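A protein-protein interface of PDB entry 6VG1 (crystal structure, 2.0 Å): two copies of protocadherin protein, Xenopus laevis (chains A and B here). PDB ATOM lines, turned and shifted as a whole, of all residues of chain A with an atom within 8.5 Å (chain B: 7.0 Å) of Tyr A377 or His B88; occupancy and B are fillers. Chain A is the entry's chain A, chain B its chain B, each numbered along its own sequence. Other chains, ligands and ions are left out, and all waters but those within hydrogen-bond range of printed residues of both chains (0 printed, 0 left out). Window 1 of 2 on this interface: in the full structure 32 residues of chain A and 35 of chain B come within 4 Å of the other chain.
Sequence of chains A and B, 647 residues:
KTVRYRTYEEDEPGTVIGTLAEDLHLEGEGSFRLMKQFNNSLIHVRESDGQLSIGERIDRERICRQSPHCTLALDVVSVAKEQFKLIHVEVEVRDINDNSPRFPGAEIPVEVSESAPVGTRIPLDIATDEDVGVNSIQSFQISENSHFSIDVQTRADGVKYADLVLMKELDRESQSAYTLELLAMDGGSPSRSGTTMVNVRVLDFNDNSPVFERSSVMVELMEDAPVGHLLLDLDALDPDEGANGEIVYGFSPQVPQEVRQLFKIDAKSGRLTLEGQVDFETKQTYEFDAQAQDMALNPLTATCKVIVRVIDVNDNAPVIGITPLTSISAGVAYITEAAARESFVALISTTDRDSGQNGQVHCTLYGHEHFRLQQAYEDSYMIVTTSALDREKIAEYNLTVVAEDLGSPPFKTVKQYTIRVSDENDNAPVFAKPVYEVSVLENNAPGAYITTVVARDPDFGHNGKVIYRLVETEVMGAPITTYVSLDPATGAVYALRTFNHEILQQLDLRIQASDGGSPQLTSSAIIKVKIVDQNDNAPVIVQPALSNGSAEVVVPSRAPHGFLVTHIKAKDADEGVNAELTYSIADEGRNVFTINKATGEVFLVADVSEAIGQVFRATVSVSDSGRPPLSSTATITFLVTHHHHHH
Of the 16 printed residues of chain A, 5 touch a printed residue of chain B. Printed residues of chain A that touch a printed residue of chain B: Phe A344, Leu A347, Ala A376, Tyr A377 and Met A382. Hydrophobic or aromatic side chains of chain A within 4 Å of the printed part of chain B: Phe A344, Leu A347, Tyr A377 and Met A382. Of the 16 printed residues of chain B, 5 touch a printed residue of chain A. Among the printed residues, 7 pairs touch across the chains.
Among the printed residues, merely in contact across the chains: Leu A347 with Asp B75, Tyr A377 with His B88, Phe A344 with Leu B86, Tyr A377 with Thr B2, Ala A376 with Lys B1 and Met A382 with Leu B86.
The side-chain hydroxyl (OH) of Tyr A377 sits at hydrogen-bond distance from the side-chain carboxylate (OD2) of Asp B75 (2.6 Å).
No position is printed for both chains. Of the 7 pairs that touch across the chains among the printed residues, none has its exchanged pair printed and touching as well.
N of Val B3 lies within hydrogen-bond range of O of His B88, at 2.9 Å. The side-chain carboxylate (OD1) of Asp B75 is in hydrogen-bond range of a ring nitrogen (ND1) of His B88 (2.5 Å). O of Lys B1 is in hydrogen-bond range of N of His B88 (3.2 Å). O of Tyr A377 lies within hydrogen-bond range of NE2 of Gln A375, at 3.3 Å. The backbone carbonyl oxygen of Thr B2 lies within hydrogen-bond range of the guanidinium group of Arg B4 (3.5 Å). The backbone carbonyl oxygen (O) of Gln A374 is in hydrogen-bond range of the backbone NH (N) of Met A382, at 2.4 Å.
Of chain B, only Thr B2 (3.9 Å), Asp B75 (2.6 Å) and His B88 (3.3 Å) come within 4 Å of Tyr A377. His B88 touches one residue of chain A. Printed residues of chain A within 4 Å of Thr B2: Tyr A377. Of the printed residues of chain B, Met A382 touches Leu B86 (3.98 Å). Of the printed residues of chain A, Lys B1 touches Ala A376 (3.9 Å). The nearest residue of chain B that does not touch Tyr A377 is Leu B86 (5.0 Å). The nearest residue of chain A that does not touch His B88 is Ala A376 (5.3 Å).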
ATOM      1  N   THR A 323     -13.592  10.466 -11.651  1.00  0.00           N
ATOM      2  CA  THR A 323     -13.160   9.967 -12.953  1.00  0.00           C
ATOM      3  C   THR A 323     -12.598  11.100 -13.800  1.00  0.00           C
ATOM      4  O   THR A 323     -13.334  12.054 -14.119  1.00  0.00           O
ATOM      5  CB  THR A 323     -14.325   9.278 -13.667  1.00  0.00           C
ATOM      6  OG1 THR A 323     -13.918   8.878 -14.980  1.00  0.00           O
ATOM      7  CG2 THR A 323     -15.544  10.192 -13.770  1.00  0.00           C
ATOM      8  N   PHE A 344     -13.530  21.403 -18.187  1.00  0.00           N
ATOM      9  CA  PHE A 344     -13.818  20.248 -17.352  1.00  0.00           C
ATOM     10  C   PHE A 344     -12.546  19.426 -17.169  1.00  0.00           C
ATOM     11  O   PHE A 344     -11.860  19.106 -18.145  1.00  0.00           O
ATOM     12  CB  PHE A 344     -14.942  19.442 -18.005  1.00  0.00           C
ATOM     13  CG  PHE A 344     -14.953  18.008 -17.635  1.00  0.00           C
ATOM     14  CD1 PHE A 344     -15.736  17.548 -16.591  1.00  0.00           C
ATOM     15  CD2 PHE A 344     -14.192  17.103 -18.350  1.00  0.00           C
ATOM     16  CE1 PHE A 344     -15.743  16.212 -16.255  1.00  0.00           C
ATOM     17  CE2 PHE A 344     -14.196  15.760 -18.018  1.00  0.00           C
ATOM     18  CZ  PHE A 344     -14.969  15.315 -16.975  1.00  0.00           C
ATOM     19  N   LEU A 347     -14.771  14.427 -13.190  1.00  0.00           N
ATOM     20  CA  LEU A 347     -16.152  14.365 -12.738  1.00  0.00           C
ATOM     21  C   LEU A 347     -16.229  13.625 -11.412  1.00  0.00           C
ATOM     22  O   LEU A 347     -15.705  12.510 -11.280  1.00  0.00           O
ATOM     23  CB  LEU A 347     -17.036  13.675 -13.778  1.00  0.00           C
ATOM     24  CG  LEU A 347     -18.516  13.536 -13.416  1.00  0.00           C
ATOM     25  CD1 LEU A 347     -19.173  14.909 -13.334  1.00  0.00           C
ATOM     26  CD2 LEU A 347     -19.238  12.640 -14.417  1.00  0.00           C
ATOM     27  N   ILE A 348     -16.894  14.247 -10.443  1.00  0.00           N
ATOM     28  CA  ILE A 348     -17.040  13.699  -9.102  1.00  0.00           C
ATOM     29  C   ILE A 348     -18.460  13.193  -8.929  1.00  0.00           C
ATOM     30  O   ILE A 348     -19.425  13.909  -9.225  1.00  0.00           O
ATOM     31  CB  ILE A 348     -16.740  14.745  -8.020  1.00  0.00           C
ATOM     32  CG1 ILE A 348     -15.348  15.325  -8.187  1.00  0.00           C
ATOM     33  CG2 ILE A 348     -16.867  14.130  -6.630  1.00  0.00           C
ATOM     34  CD1 ILE A 348     -15.108  16.559  -7.345  1.00  0.00           C
ATOM     35  N   SER A 349     -18.581  11.959  -8.468  1.00  0.00           N
ATOM     36  CA  SER A 349     -19.852  11.352  -8.111  1.00  0.00           C
ATOM     37  C   SER A 349     -19.901  11.223  -6.595  1.00  0.00           C
ATOM     38  O   SER A 349     -18.998  10.632  -5.989  1.00  0.00           O
ATOM     39  CB  SER A 349     -20.017   9.977  -8.757  1.00  0.00           C
ATOM     40  OG  SER A 349     -21.151   9.321  -8.209  1.00  0.00           O
ATOM     41  N   THR A 350     -20.938  11.783  -5.984  1.00  0.00           N
ATOM     42  CA  THR A 350     -21.180  11.647  -4.553  1.00  0.00           C
ATOM     43  C   THR A 350     -22.538  10.984  -4.396  1.00  0.00           C
ATOM     44  O   THR A 350     -23.563  11.591  -4.729  1.00  0.00           O
ATOM     45  CB  THR A 350     -21.140  13.002  -3.867  1.00  0.00           C
ATOM     46  OG1 THR A 350     -22.071  13.876  -4.507  1.00  0.00           O
ATOM     47  CG2 THR A 350     -19.759  13.577  -3.993  1.00  0.00           C
ATOM     48  N   VAL A 361     -26.873  14.187  -0.614  1.00  0.00           N
ATOM     49  CA  VAL A 361     -25.458  14.476  -0.417  1.00  0.00           C
ATOM     50  C   VAL A 361     -25.138  15.917  -0.785  1.00  0.00           C
ATOM     51  O   VAL A 361     -25.606  16.438  -1.805  1.00  0.00           O
ATOM     52  CB  VAL A 361     -24.560  13.528  -1.232  1.00  0.00           C
ATOM     53  CG1 VAL A 361     -24.804  12.092  -0.848  1.00  0.00           C
ATOM     54  CG2 VAL A 361     -24.796  13.736  -2.732  1.00  0.00           C
ATOM     55  N   GLN A 374     -18.667  22.462 -10.187  1.00  0.00           N
ATOM     56  CA  GLN A 374     -19.819  22.799 -11.015  1.00  0.00           C
ATOM     57  C   GLN A 374     -20.690  21.559 -11.144  1.00  0.00           C
ATOM     58  O   GLN A 374     -20.236  20.533 -11.662  1.00  0.00           O
ATOM     59  CB  GLN A 374     -19.376  23.294 -12.391  1.00  0.00           C
ATOM     60  CG  GLN A 374     -20.510  23.832 -13.242  1.00  0.00           C
ATOM     61  CD  GLN A 374     -21.290  24.933 -12.550  1.00  0.00           C
ATOM     62  OE1 GLN A 374     -20.710  25.857 -11.979  1.00  0.00           O
ATOM     63  NE2 GLN A 374     -22.614  24.831 -12.591  1.00  0.00           N
ATOM     64  N   GLN A 375     -21.932  21.646 -10.675  1.00  0.00           N
ATOM     65  CA  GLN A 375     -22.812  20.484 -10.717  1.00  0.00           C
ATOM     66  C   GLN A 375     -23.235  20.227 -12.160  1.00  0.00           C
ATOM     67  O   GLN A 375     -23.781  21.116 -12.821  1.00  0.00           O
ATOM     68  CB  GLN A 375     -24.040  20.677  -9.821  1.00  0.00           C
ATOM     69  CG  GLN A 375     -24.913  19.413  -9.713  1.00  0.00           C
ATOM     70  CD  GLN A 375     -25.864  19.419  -8.532  1.00  0.00           C
ATOM     71  OE1 GLN A 375     -25.888  20.364  -7.738  1.00  0.00           O
ATOM     72  NE2 GLN A 375     -26.657  18.350  -8.407  1.00  0.00           N
ATOM     73  N   ALA A 376     -23.004  19.001 -12.634  1.00  0.00           N
ATOM     74  CA  ALA A 376     -23.392  18.591 -13.978  1.00  0.00           C
ATOM     75  C   ALA A 376     -24.771  17.944 -13.980  1.00  0.00           C
ATOM     76  O   ALA A 376     -25.611  18.267 -14.828  1.00  0.00           O
ATOM     77  CB  ALA A 376     -22.343  17.635 -14.552  1.00  0.00           C
ATOM     78  N   TYR A 377     -25.020  17.030 -13.047  1.00  0.00           N
ATOM     79  CA  TYR A 377     -26.348  16.426 -12.925  1.00  0.00           C
ATOM     80  C   TYR A 377     -26.485  15.856 -11.518  1.00  0.00           C
ATOM     81  O   TYR A 377     -25.668  16.143 -10.637  1.00  0.00           O
ATOM     82  CB  TYR A 377     -26.590  15.377 -14.022  1.00  0.00           C
ATOM     83  CG  TYR A 377     -25.508  14.332 -14.197  1.00  0.00           C
ATOM     84  CD1 TYR A 377     -25.683  13.045 -13.725  1.00  0.00           C
ATOM     85  CD2 TYR A 377     -24.328  14.629 -14.863  1.00  0.00           C
ATOM     86  CE1 TYR A 377     -24.712  12.086 -13.893  1.00  0.00           C
ATOM     87  CE2 TYR A 377     -23.343  13.677 -15.034  1.00  0.00           C
ATOM     88  CZ  TYR A 377     -23.538  12.401 -14.547  1.00  0.00           C
ATOM     89  OH  TYR A 377     -22.558  11.439 -14.711  1.00  0.00           O
ATOM     90  N   GLU A 378     -27.524  15.050 -11.297  1.00  0.00           N
ATOM     91  CA  GLU A 378     -27.810  14.577  -9.946  1.00  0.00           C
ATOM     92  C   GLU A 378     -26.582  13.881  -9.365  1.00  0.00           C
ATOM     93  O   GLU A 378     -26.018  12.964  -9.972  1.00  0.00           O
ATOM     94  CB  GLU A 378     -29.016  13.634  -9.943  1.00  0.00           C
ATOM     95  CG  GLU A 378     -29.482  13.226  -8.532  1.00  0.00           C
ATOM     96  CD  GLU A 378     -30.733  12.362  -8.539  1.00  0.00           C
ATOM     97  OE1 GLU A 378     -31.282  12.095  -9.630  1.00  0.00           O
ATOM     98  OE2 GLU A 378     -31.171  11.944  -7.447  1.00  0.00           O
ATOM     99  N   ASP A 379     -26.151  14.341  -8.193  1.00  0.00           N
ATOM    100  CA  ASP A 379     -25.032  13.728  -7.475  1.00  0.00           C
ATOM    101  C   ASP A 379     -23.783  13.628  -8.353  1.00  0.00           C
ATOM    102  O   ASP A 379     -22.913  12.786  -8.129  1.00  0.00           O
ATOM    103  CB  ASP A 379     -25.420  12.347  -6.931  1.00  0.00           C
ATOM    104  CG  ASP A 379     -26.459  12.420  -5.829  1.00  0.00           C
ATOM    105  OD1 ASP A 379     -26.489  13.432  -5.101  1.00  0.00           O
ATOM    106  OD2 ASP A 379     -27.230  11.451  -5.667  1.00  0.00           O
ATOM    107  N   SER A 380     -23.655  14.512  -9.335  1.00  0.00           N
ATOM    108  CA  SER A 380     -22.502  14.487 -10.231  1.00  0.00           C
ATOM    109  C   SER A 380     -22.024  15.909 -10.471  1.00  0.00           C
ATOM    110  O   SER A 380     -22.697  16.691 -11.158  1.00  0.00           O
ATOM    111  CB  SER A 380     -22.842  13.789 -11.546  1.00  0.00           C
ATOM    112  OG  SER A 380     -22.930  12.385 -11.340  1.00  0.00           O
ATOM    113  N   TYR A 381     -20.857  16.218  -9.907  1.00  0.00           N
ATOM    114  CA  TYR A 381     -20.278  17.549  -9.884  1.00  0.00           C
ATOM    115  C   TYR A 381     -18.983  17.541 -10.677  1.00  0.00           C
ATOM    116  O   TYR A 381     -18.183  16.608 -10.563  1.00  0.00           O
ATOM    117  CB  TYR A 381     -19.990  17.993  -8.448  1.00  0.00           C
ATOM    118  CG  TYR A 381     -21.207  17.964  -7.542  1.00  0.00           C
ATOM    119  CD1 TYR A 381     -21.879  19.142  -7.214  1.00  0.00           C
ATOM    120  CD2 TYR A 381     -21.687  16.769  -7.026  1.00  0.00           C
ATOM    121  CE1 TYR A 381     -22.979  19.134  -6.394  1.00  0.00           C
ATOM    122  CE2 TYR A 381     -22.793  16.750  -6.207  1.00  0.00           C
ATOM    123  CZ  TYR A 381     -23.438  17.939  -5.892  1.00  0.00           C
ATOM    124  OH  TYR A 381     -24.545  17.922  -5.069  1.00  0.00           O
ATOM    125  N   MET A 382     -18.784  18.582 -11.475  1.00  0.00           N
ATOM    126  CA  MET A 382     -17.581  18.716 -12.281  1.00  0.00           C
ATOM    127  C   MET A 382     -16.558  19.576 -11.556  1.00  0.00           C
ATOM    128  O   MET A 382     -16.915  20.548 -10.885  1.00  0.00           O
ATOM    129  CB  MET A 382     -17.885  19.360 -13.633  1.00  0.00           C
ATOM    130  CG  MET A 382     -18.716  18.530 -14.586  1.00  0.00           C
ATOM    131  SD  MET A 382     -18.954  19.427 -16.144  1.00  0.00           S
ATOM    132  CE  MET A 382     -20.050  20.744 -15.641  1.00  0.00           C
ATOM    133  N   LYS B   1     -25.020  19.677 -18.427  1.00  0.00           N
ATOM    134  CA  LYS B   1     -26.473  19.685 -18.774  1.00  0.00           C
ATOM    135  C   LYS B   1     -26.904  18.321 -19.310  1.00  0.00           C
ATOM    136  O   LYS B   1     -26.097  17.595 -19.891  1.00  0.00           O
ATOM    137  CB  LYS B   1     -26.768  20.778 -19.799  1.00  0.00           C
ATOM    138  CG  LYS B   1     -26.488  22.198 -19.308  1.00  0.00           C
ATOM    139  CD  LYS B   1     -26.774  23.213 -20.410  1.00  0.00           C
ATOM    140  CE  LYS B   1     -26.457  24.636 -19.969  1.00  0.00           C
ATOM    141  NZ  LYS B   1     -26.719  25.611 -21.075  1.00  0.00           N
ATOM    142  N   THR B   2     -28.179  17.977 -19.124  1.00  0.00           N
ATOM    143  CA  THR B   2     -28.691  16.656 -19.480  1.00  0.00           C
ATOM    144  C   THR B   2     -29.494  16.751 -20.773  1.00  0.00           C
ATOM    145  O   THR B   2     -30.577  17.351 -20.799  1.00  0.00           O
ATOM    146  CB  THR B   2     -29.548  16.088 -18.348  1.00  0.00           C
ATOM    147  OG1 THR B   2     -28.822  16.149 -17.113  1.00  0.00           O
ATOM    148  CG2 THR B   2     -29.930  14.642 -18.629  1.00  0.00           C
ATOM    149  N   VAL B   3     -28.968  16.136 -21.842  1.00  0.00           N
ATOM    150  CA  VAL B   3     -29.631  16.072 -23.141  1.00  0.00           C
ATOM    151  C   VAL B   3     -30.253  14.698 -23.318  1.00  0.00           C
ATOM    152  O   VAL B   3     -29.620  13.673 -23.029  1.00  0.00           O
ATOM    153  CB  VAL B   3     -28.647  16.372 -24.286  1.00  0.00           C
ATOM    154  CG1 VAL B   3     -27.496  15.386 -24.287  1.00  0.00           C
ATOM    155  CG2 VAL B   3     -29.383  16.325 -25.622  1.00  0.00           C
ATOM    156  N   ARG B   4     -31.481  14.670 -23.828  1.00  0.00           N
ATOM    157  CA  ARG B   4     -32.316  13.480 -23.781  1.00  0.00           C
ATOM    158  C   ARG B   4     -32.629  12.968 -25.174  1.00  0.00           C
ATOM    159  O   ARG B   4     -33.033  13.735 -26.055  1.00  0.00           O
ATOM    160  CB  ARG B   4     -33.621  13.772 -23.037  1.00  0.00           C
ATOM    161  CG  ARG B   4     -33.440  14.016 -21.550  1.00  0.00           C
ATOM    162  CD  ARG B   4     -34.755  14.331 -20.871  1.00  0.00           C
ATOM    163  NE  ARG B   4     -34.588  14.454 -19.429  1.00  0.00           N
ATOM    164  CZ  ARG B   4     -34.115  15.539 -18.823  1.00  0.00           C
ATOM    165  NH1 ARG B   4     -33.753  16.601 -19.536  1.00  0.00           N
ATOM    166  NH2 ARG B   4     -33.997  15.563 -17.501  1.00  0.00           N
ATOM    167  N   LEU B  20     -25.423  15.414 -31.323  1.00  0.00           N
ATOM    168  CA  LEU B  20     -25.196  16.439 -30.309  1.00  0.00           C
ATOM    169  C   LEU B  20     -24.820  17.770 -30.946  1.00  0.00           C
ATOM    170  O   LEU B  20     -25.412  18.809 -30.627  1.00  0.00           O
ATOM    171  CB  LEU B  20     -24.112  15.982 -29.333  1.00  0.00           C
ATOM    172  CG  LEU B  20     -24.487  14.811 -28.428  1.00  0.00           C
ATOM    173  CD1 LEU B  20     -23.227  14.259 -27.758  1.00  0.00           C
ATOM    174  CD2 LEU B  20     -25.517  15.197 -27.394  1.00  0.00           C
ATOM    175  N   LYS B  36     -15.890   6.783 -20.052  1.00  0.00           N
ATOM    176  CA  LYS B  36     -15.816   5.441 -19.495  1.00  0.00           C
ATOM    177  C   LYS B  36     -15.724   4.413 -20.615  1.00  0.00           C
ATOM    178  O   LYS B  36     -16.653   4.275 -21.416  1.00  0.00           O
ATOM    179  CB  LYS B  36     -17.040   5.137 -18.633  1.00  0.00           C
ATOM    180  CG  LYS B  36     -17.245   6.033 -17.429  1.00  0.00           C
ATOM    181  CD  LYS B  36     -18.599   5.711 -16.787  1.00  0.00           C
ATOM    182  CE  LYS B  36     -18.842   6.491 -15.511  1.00  0.00           C
ATOM    183  NZ  LYS B  36     -20.174   6.143 -14.930  1.00  0.00           N
ATOM    184  N   LEU B  72     -30.265   4.735 -20.387  1.00  0.00           N
ATOM    185  CA  LEU B  72     -28.819   4.586 -20.389  1.00  0.00           C
ATOM    186  C   LEU B  72     -28.171   5.958 -20.271  1.00  0.00           C
ATOM    187  O   LEU B  72     -28.517   6.878 -21.015  1.00  0.00           O
ATOM    188  CB  LEU B  72     -28.350   3.887 -21.663  1.00  0.00           C
ATOM    189  CG  LEU B  72     -28.432   2.363 -21.637  1.00  0.00           C
ATOM    190  CD1 LEU B  72     -28.062   1.826 -22.999  1.00  0.00           C
ATOM    191  CD2 LEU B  72     -27.532   1.805 -20.556  1.00  0.00           C
ATOM    192  N   ALA B  73     -27.228   6.093 -19.345  1.00  0.00           N
ATOM    193  CA  ALA B  73     -26.552   7.358 -19.096  1.00  0.00           C
ATOM    194  C   ALA B  73     -25.142   7.304 -19.660  1.00  0.00           C
ATOM    195  O   ALA B  73     -24.395   6.360 -19.385  1.00  0.00           O
ATOM    196  CB  ALA B  73     -26.509   7.668 -17.601  1.00  0.00           C
ATOM    197  N   LEU B  74     -24.782   8.312 -20.450  1.00  0.00           N
ATOM    198  CA  LEU B  74     -23.444   8.393 -21.021  1.00  0.00           C
ATOM    199  C   LEU B  74     -22.918   9.814 -20.889  1.00  0.00           C
ATOM    200  O   LEU B  74     -23.652  10.779 -21.104  1.00  0.00           O
ATOM    201  CB  LEU B  74     -23.430   7.970 -22.496  1.00  0.00           C
ATOM    202  CG  LEU B  74     -23.824   6.521 -22.767  1.00  0.00           C
ATOM    203  CD1 LEU B  74     -23.967   6.301 -24.273  1.00  0.00           C
ATOM    204  CD2 LEU B  74     -22.817   5.549 -22.180  1.00  0.00           C
ATOM    205  N   ASP B  75     -21.638   9.936 -20.543  1.00  0.00           N
ATOM    206  CA  ASP B  75     -20.987  11.229 -20.380  1.00  0.00           C
ATOM    207  C   ASP B  75     -19.972  11.413 -21.501  1.00  0.00           C
ATOM    208  O   ASP B  75     -18.987  10.671 -21.578  1.00  0.00           O
ATOM    209  CB  ASP B  75     -20.303  11.332 -19.016  1.00  0.00           C
ATOM    210  CG  ASP B  75     -21.292  11.440 -17.865  1.00  0.00           C
ATOM    211  OD1 ASP B  75     -22.458  11.823 -18.099  1.00  0.00           O
ATOM    212  OD2 ASP B  75     -20.894  11.144 -16.717  1.00  0.00           O
ATOM    213  N   VAL B  76     -20.210  12.399 -22.364  1.00  0.00           N
ATOM    214  CA  VAL B  76     -19.332  12.669 -23.497  1.00  0.00           C
ATOM    215  C   VAL B  76     -18.580  13.962 -23.219  1.00  0.00           C
ATOM    216  O   VAL B  76     -19.088  14.867 -22.553  1.00  0.00           O
ATOM    217  CB  VAL B  76     -20.117  12.770 -24.822  1.00  0.00           C
ATOM    218  CG1 VAL B  76     -20.764  11.450 -25.153  1.00  0.00           C
ATOM    219  CG2 VAL B  76     -21.143  13.887 -24.721  1.00  0.00           C
ATOM    220  N   LEU B  86     -18.174  18.980 -21.057  1.00  0.00           N
ATOM    221  CA  LEU B  86     -18.803  17.694 -20.794  1.00  0.00           C
ATOM    222  C   LEU B  86     -20.311  17.809 -20.949  1.00  0.00           C
ATOM    223  O   LEU B  86     -20.927  18.770 -20.475  1.00  0.00           O
ATOM    224  CB  LEU B  86     -18.467  17.175 -19.387  1.00  0.00           C
ATOM    225  CG  LEU B  86     -19.180  15.889 -18.999  1.00  0.00           C
ATOM    226  CD1 LEU B  86     -18.311  15.019 -18.103  1.00  0.00           C
ATOM    227  CD2 LEU B  86     -20.501  16.178 -18.288  1.00  0.00           C
ATOM    228  N   ILE B  87     -20.900  16.810 -21.596  1.00  0.00           N
ATOM    229  CA  ILE B  87     -22.338  16.743 -21.823  1.00  0.00           C
ATOM    230  C   ILE B  87     -22.839  15.400 -21.312  1.00  0.00           C
ATOM    231  O   ILE B  87     -22.313  14.347 -21.689  1.00  0.00           O
ATOM    232  CB  ILE B  87     -22.704  16.917 -23.308  1.00  0.00           C
ATOM    233  CG1 ILE B  87     -21.951  18.104 -23.895  1.00  0.00           C
ATOM    234  CG2 ILE B  87     -24.201  17.118 -23.465  1.00  0.00           C
ATOM    235  CD1 ILE B  87     -22.445  18.550 -25.262  1.00  0.00           C
ATOM    236  N   HIS B  88     -23.835  15.445 -20.433  1.00  0.00           N
ATOM    237  CA  HIS B  88     -24.471  14.262 -19.877  1.00  0.00           C
ATOM    238  C   HIS B  88     -25.704  13.939 -20.704  1.00  0.00           C
ATOM    239  O   HIS B  88     -26.535  14.819 -20.952  1.00  0.00           O
ATOM    240  CB  HIS B  88     -24.858  14.501 -18.419  1.00  0.00           C
ATOM    241  CG  HIS B  88     -25.536  13.334 -17.783  1.00  0.00           C
ATOM    242  ND1 HIS B  88     -24.899  12.130 -17.568  1.00  0.00           N
ATOM    243  CD2 HIS B  88     -26.800  13.178 -17.325  1.00  0.00           C
ATOM    244  CE1 HIS B  88     -25.740  11.287 -16.999  1.00  0.00           C
ATOM    245  NE2 HIS B  88     -26.900  11.898 -16.840  1.00  0.00           N
ATOM    246  N   VAL B  89     -25.826  12.686 -21.133  1.00  0.00           N
ATOM    247  CA  VAL B  89     -26.899  12.290 -22.032  1.00  0.00           C
ATOM    248  C   VAL B  89     -27.634  11.090 -21.460  1.00  0.00           C
ATOM    249  O   VAL B  89     -27.012  10.134 -20.981  1.00  0.00           O
ATOM    250  CB  VAL B  89     -26.370  11.961 -23.440  1.00  0.00           C
ATOM    251  CG1 VAL B  89     -25.382  10.807 -23.375  1.00  0.00           C
ATOM    252  CG2 VAL B  89     -27.529  11.605 -24.360  1.00  0.00           C
ATOM    253  N   GLU B  90     -28.962  11.142 -21.532  1.00  0.00           N
ATOM    254  CA  GLU B  90     -29.844  10.073 -21.081  1.00  0.00           C
ATOM    255  C   GLU B  90     -30.617   9.555 -22.285  1.00  0.00           C
ATOM    256  O   GLU B  90     -31.402  10.295 -22.888  1.00  0.00           O
ATOM    257  CB  GLU B  90     -30.787  10.574 -19.983  1.00  0.00           C
ATOM    258  CG  GLU B  90     -30.108  10.701 -18.622  1.00  0.00           C
ATOM    259  CD  GLU B  90     -30.927  11.480 -17.603  1.00  0.00           C
ATOM    260  OE1 GLU B  90     -32.031  11.947 -17.953  1.00  0.00           O
ATOM    261  OE2 GLU B  90     -30.456  11.629 -16.451  1.00  0.00           O
